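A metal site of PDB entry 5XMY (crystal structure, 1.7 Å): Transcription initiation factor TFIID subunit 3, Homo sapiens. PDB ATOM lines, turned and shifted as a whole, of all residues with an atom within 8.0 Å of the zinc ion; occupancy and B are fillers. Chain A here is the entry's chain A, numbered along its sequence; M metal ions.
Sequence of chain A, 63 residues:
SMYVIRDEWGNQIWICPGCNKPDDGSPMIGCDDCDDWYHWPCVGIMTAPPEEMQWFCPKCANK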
ATOM      1  N   PRO A  17      25.848   5.037  -1.826  1.00  0.00           N
ATOM      2  CA  PRO A  17      24.663   5.419  -1.039  1.00  0.00           C
ATOM      3  C   PRO A  17      24.928   6.519  -0.035  1.00  0.00           C
ATOM      4  O   PRO A  17      23.962   7.159   0.435  1.00  0.00           O
ATOM      5  CB  PRO A  17      24.290   4.117  -0.313  1.00  0.00           C
ATOM      6  CG  PRO A  17      24.856   3.020  -1.186  1.00  0.00           C
ATOM      7  CD  PRO A  17      26.172   3.616  -1.637  1.00  0.00           C
ATOM      8  N   GLY A  30      33.215  -2.374  -0.647  1.00  0.00           N
ATOM      9  CA  GLY A  30      31.976  -3.077  -0.889  1.00  0.00           C
ATOM     10  C   GLY A  30      31.458  -3.727   0.382  1.00  0.00           C
ATOM     11  O   GLY A  30      32.214  -4.400   1.106  1.00  0.00           O
ATOM     12  N   CYS A  31      30.176  -3.532   0.634  1.00  0.00           N
ATOM     13  CA  CYS A  31      29.562  -4.096   1.845  1.00  0.00           C
ATOM     14  C   CYS A  31      29.358  -5.596   1.707  1.00  0.00           C
ATOM     15  O   CYS A  31      28.777  -6.074   0.733  1.00  0.00           O
ATOM     16  CB  CYS A  31      28.233  -3.386   2.105  1.00  0.00           C
ATOM     17  SG  CYS A  31      27.416  -4.058   3.580  1.00  0.00           S
ATOM     18  N   ASP A  32      29.867  -6.353   2.675  1.00  0.00           N
ATOM     19  CA  ASP A  32      29.804  -7.809   2.613  1.00  0.00           C
ATOM     20  C   ASP A  32      28.472  -8.376   3.039  1.00  0.00           C
ATOM     21  O   ASP A  32      28.324  -9.596   3.122  1.00  0.00           O
ATOM     22  CB  ASP A  32      30.930  -8.377   3.463  1.00  0.00           C
ATOM     23  CG  ASP A  32      32.270  -8.177   2.802  1.00  0.00           C
ATOM     24  OD1 ASP A  32      32.331  -8.389   1.580  1.00  0.00           O
ATOM     25  OD2 ASP A  32      33.238  -7.758   3.476  1.00  0.00           O
ATOM     26  N   ASP A  33      27.487  -7.510   3.302  1.00  0.00           N
ATOM     27  CA  ASP A  33      26.107  -7.908   3.509  1.00  0.00           C
ATOM     28  C   ASP A  33      25.295  -7.548   2.267  1.00  0.00           C
ATOM     29  O   ASP A  33      24.870  -8.431   1.521  1.00  0.00           O
ATOM     30  CB  ASP A  33      25.564  -7.206   4.753  1.00  0.00           C
ATOM     31  CG  ASP A  33      24.169  -7.666   5.128  1.00  0.00           C
ATOM     32  OD1 ASP A  33      23.430  -8.217   4.273  1.00  0.00           O
ATOM     33  OD2 ASP A  33      23.811  -7.450   6.306  1.00  0.00           O
ATOM     34  N   CYS A  34      25.062  -6.251   2.053  1.00  0.00           N
ATOM     35  CA  CYS A  34      24.147  -5.805   1.009  1.00  0.00           C
ATOM     36  C   CYS A  34      24.774  -5.661  -0.375  1.00  0.00           C
ATOM     37  O   CYS A  34      24.039  -5.609  -1.364  1.00  0.00           O
ATOM     38  CB  CYS A  34      23.500  -4.462   1.388  1.00  0.00           C
ATOM     39  SG  CYS A  34      24.594  -2.995   1.314  1.00  0.00           S
ATOM     40  N   ASP A  35      26.104  -5.583  -0.463  1.00  0.00           N
ATOM     41  CA  ASP A  35      26.909  -5.492  -1.690  1.00  0.00           C
ATOM     42  C   ASP A  35      26.857  -4.123  -2.367  1.00  0.00           C
ATOM     43  O   ASP A  35      27.322  -3.993  -3.539  1.00  0.00           O
ATOM     44  CB  ASP A  35      26.523  -6.569  -2.706  1.00  0.00           C
ATOM     45  CG  ASP A  35      27.657  -6.883  -3.661  1.00  0.00           C
ATOM     46  OD1 ASP A  35      28.821  -6.548  -3.333  1.00  0.00           O
ATOM     47  OD2 ASP A  35      27.386  -7.446  -4.746  1.00  0.00           O
ATOM     48  N   ASP A  36      26.321  -3.092  -1.707  1.00  0.00           N
ATOM     49  CA  ASP A  36      26.521  -1.724  -2.205  1.00  0.00           C
ATOM     50  C   ASP A  36      27.975  -1.308  -2.029  1.00  0.00           C
ATOM     51  O   ASP A  36      28.693  -1.783  -1.125  1.00  0.00           O
ATOM     52  CB  ASP A  36      25.609  -0.721  -1.470  1.00  0.00           C
ATOM     53  CG  ASP A  36      24.119  -0.923  -1.777  1.00  0.00           C
ATOM     54  OD1 ASP A  36      23.761  -1.467  -2.846  1.00  0.00           O
ATOM     55  OD2 ASP A  36      23.300  -0.532  -0.903  1.00  0.00           O
ATOM     56  N   TRP A  37      28.420  -0.393  -2.877  1.00  0.00           N
ATOM     57  CA  TRP A  37      29.785   0.119  -2.848  1.00  0.00           C
ATOM     58  C   TRP A  37      29.807   1.571  -2.427  1.00  0.00           C
ATOM     59  O   TRP A  37      28.985   2.382  -2.892  1.00  0.00           O
ATOM     60  CB  TRP A  37      30.444  -0.033  -4.224  1.00  0.00           C
ATOM     61  CG  TRP A  37      30.862  -1.440  -4.510  1.00  0.00           C
ATOM     62  CD1 TRP A  37      30.063  -2.452  -4.944  1.00  0.00           C
ATOM     63  CD2 TRP A  37      32.174  -1.998  -4.352  1.00  0.00           C
ATOM     64  NE1 TRP A  37      30.809  -3.617  -5.080  1.00  0.00           N
ATOM     65  CE2 TRP A  37      32.105  -3.351  -4.728  1.00  0.00           C
ATOM     66  CE3 TRP A  37      33.401  -1.460  -3.951  1.00  0.00           C
ATOM     67  CZ2 TRP A  37      33.232  -4.190  -4.688  1.00  0.00           C
ATOM     68  CZ3 TRP A  37      34.515  -2.287  -3.936  1.00  0.00           C
ATOM     69  CH2 TRP A  37      34.417  -3.635  -4.299  1.00  0.00           C
ATOM     70  N   TYR A  38      30.741   1.910  -1.543  1.00  0.00           N
ATOM     71  CA  TYR A  38      30.860   3.237  -0.960  1.00  0.00           C
ATOM     72  C   TYR A  38      32.233   3.833  -1.213  1.00  0.00           C
ATOM     73  O   TYR A  38      33.256   3.129  -1.174  1.00  0.00           O
ATOM     74  CB  TYR A  38      30.638   3.250   0.558  1.00  0.00           C
ATOM     75  CG  TYR A  38      29.227   3.001   1.023  1.00  0.00           C
ATOM     76  CD1 TYR A  38      28.650   1.734   0.951  1.00  0.00           C
ATOM     77  CD2 TYR A  38      28.463   4.037   1.566  1.00  0.00           C
ATOM     78  CE1 TYR A  38      27.352   1.513   1.379  1.00  0.00           C
ATOM     79  CE2 TYR A  38      27.168   3.815   2.019  1.00  0.00           C
ATOM     80  CZ  TYR A  38      26.615   2.554   1.919  1.00  0.00           C
ATOM     81  OH  TYR A  38      25.331   2.336   2.345  1.00  0.00           O
ATOM     82  N   TRP A  55      33.777  -6.040   5.761  1.00  0.00           N
ATOM     83  CA  TRP A  55      33.347  -4.692   6.039  1.00  0.00           C
ATOM     84  C   TRP A  55      31.854  -4.604   5.765  1.00  0.00           C
ATOM     85  O   TRP A  55      31.368  -5.171   4.781  1.00  0.00           O
ATOM     86  CB  TRP A  55      34.104  -3.650   5.192  1.00  0.00           C
ATOM     87  CG  TRP A  55      33.628  -2.246   5.424  1.00  0.00           C
ATOM     88  CD1 TRP A  55      33.993  -1.409   6.446  1.00  0.00           C
ATOM     89  CD2 TRP A  55      32.667  -1.529   4.638  1.00  0.00           C
ATOM     90  NE1 TRP A  55      33.337  -0.215   6.337  1.00  0.00           N
ATOM     91  CE2 TRP A  55      32.513  -0.253   5.231  1.00  0.00           C
ATOM     92  CE3 TRP A  55      31.936  -1.836   3.491  1.00  0.00           C
ATOM     93  CZ2 TRP A  55      31.655   0.717   4.710  1.00  0.00           C
ATOM     94  CZ3 TRP A  55      31.073  -0.879   2.974  1.00  0.00           C
ATOM     95  CH2 TRP A  55      30.946   0.387   3.590  1.00  0.00           C
ATOM     96  N   PHE A  56      31.129  -3.942   6.666  1.00  0.00           N
ATOM     97  CA  PHE A  56      29.711  -3.730   6.501  1.00  0.00           C
ATOM     98  C   PHE A  56      29.394  -2.249   6.577  1.00  0.00           C
ATOM     99  O   PHE A  56      29.978  -1.518   7.388  1.00  0.00           O
ATOM    100  CB  PHE A  56      28.932  -4.527   7.550  1.00  0.00           C
ATOM    101  CG  PHE A  56      29.283  -5.965   7.555  1.00  0.00           C
ATOM    102  CD1 PHE A  56      28.709  -6.836   6.648  1.00  0.00           C
ATOM    103  CD2 PHE A  56      30.240  -6.447   8.448  1.00  0.00           C
ATOM    104  CE1 PHE A  56      29.057  -8.180   6.653  1.00  0.00           C
ATOM    105  CE2 PHE A  56      30.593  -7.789   8.440  1.00  0.00           C
ATOM    106  CZ  PHE A  56      29.988  -8.648   7.539  1.00  0.00           C
ATOM    107  N   CYS A  57      28.482  -1.797   5.711  1.00  0.00           N
ATOM    108  CA  CYS A  57      28.138  -0.390   5.612  1.00  0.00           C
ATOM    109  C   CYS A  57      27.322   0.025   6.827  1.00  0.00           C
ATOM    110  O   CYS A  57      26.828  -0.829   7.567  1.00  0.00           O
ATOM    111  CB  CYS A  57      27.377  -0.115   4.321  1.00  0.00           C
ATOM    112  SG  CYS A  57      25.681  -0.759   4.253  1.00  0.00           S
ATOM    113  N   PRO A  58      27.174   1.329   7.052  1.00  0.00           N
ATOM    114  CA  PRO A  58      26.402   1.785   8.221  1.00  0.00           C
ATOM    115  C   PRO A  58      24.993   1.217   8.320  1.00  0.00           C
ATOM    116  O   PRO A  58      24.550   0.863   9.417  1.00  0.00           O
ATOM    117  CB  PRO A  58      26.386   3.309   8.028  1.00  0.00           C
ATOM    118  CG  PRO A  58      27.645   3.610   7.331  1.00  0.00           C
ATOM    119  CD  PRO A  58      27.862   2.454   6.376  1.00  0.00           C
ATOM    120  N   LYS A  59      24.279   1.122   7.200  1.00  0.00           N
ATOM    121  CA  LYS A  59      22.931   0.555   7.214  1.00  0.00           C
ATOM    122  C   LYS A  59      22.934  -0.876   7.732  1.00  0.00           C
ATOM    123  O   LYS A  59      22.148  -1.228   8.623  1.00  0.00           O
ATOM    124  CB  LYS A  59      22.348   0.624   5.804  1.00  0.00           C
ATOM    125  CG  LYS A  59      21.088  -0.180   5.589  1.00  0.00           C
ATOM    126  CD  LYS A  59      20.532   0.079   4.198  1.00  0.00           C
ATOM    127  CE  LYS A  59      20.010  -1.189   3.558  1.00  0.00           C
ATOM    128  NZ  LYS A  59      18.877  -1.778   4.323  1.00  0.00           N
ATOM    129  N   CYS A  60      23.820  -1.723   7.205  1.00  0.00           N
ATOM    130  CA  CYS A  60      23.813  -3.129   7.586  1.00  0.00           C
ATOM    131  C   CYS A  60      24.410  -3.345   8.961  1.00  0.00           C
ATOM    132  O   CYS A  60      24.034  -4.292   9.655  1.00  0.00           O
ATOM    133  CB  CYS A  60      24.594  -3.964   6.562  1.00  0.00           C
ATOM    134  SG  CYS A  60      23.895  -3.975   4.903  1.00  0.00           S
ATOM    135  N   ALA A  61      25.363  -2.498   9.357  1.00  0.00           N
ATOM    136  CA  ALA A  61      26.073  -2.718  10.614  1.00  0.00           C
ATOM    137  C   ALA A  61      25.124  -2.687  11.799  1.00  0.00           C
ATOM    138  O   ALA A  61      25.364  -3.362  12.809  1.00  0.00           O
ATOM    139  CB  ALA A  61      27.185  -1.692  10.779  1.00  0.00           C
ATOM    140  N   LYS A  63      22.181  -3.924  11.610  1.00  0.00           N
ATOM    141  CA  LYS A  63      21.215  -4.988  11.356  1.00  0.00           C
ATOM    142  C   LYS A  63      21.749  -6.346  11.820  1.00  0.00           C
ATOM    143  O   LYS A  63      21.349  -7.389  11.294  1.00  0.00           O
ATOM    144  CB  LYS A  63      20.842  -5.060   9.872  1.00  0.00           C
ATOM    145  CG  LYS A  63      20.317  -3.750   9.312  1.00  0.00           C
ATOM    146  CD  LYS A  63      19.287  -3.146  10.241  1.00  0.00           C
ATOM    147  CE  LYS A  63      19.081  -1.669   9.929  1.00  0.00           C
ATOM    148  NZ  LYS A  63      18.391  -0.948  11.045  1.00  0.00           N
ATOM    149  OXT LYS A  63      22.600  -6.434  12.716  1.00  0.00           O
HETATM  150 ZN    ZN M   1      25.361  -2.965   3.507  1.00  0.00          ZN
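The backbone NH (N) of Cys 31 is in hydrogen-bond range of the backbone carbonyl oxygen (O) of Asp 36. SG of Cys 57 lies close to OH of Tyr 38 (3.7 Å). The side-chain sulfur (SG) of Cys 60 sits close to the side-chain carboxylate (OD2) of Asp 33. The side-chain sulfur of Cys 31 lies close to the backbone NH of Asp 33. The side-chain sulfur of Cys 34 lies close to the backbone NH of Asp 36. SG of Cys 57 sits close to N of Lys 59 (3.8 Å).
The zinc ion is bound by SG of Cys 60, SG of Cys 34, SG of Cys 31 and SG of Cys 57. The zinc ion has four donor atoms within binding distance.
Of the 18 residues printed, 4 come within 4 Å of the zinc ion. The nearest printed residue that does not touch the zinc ion is Asp 33 (4.4 Å).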
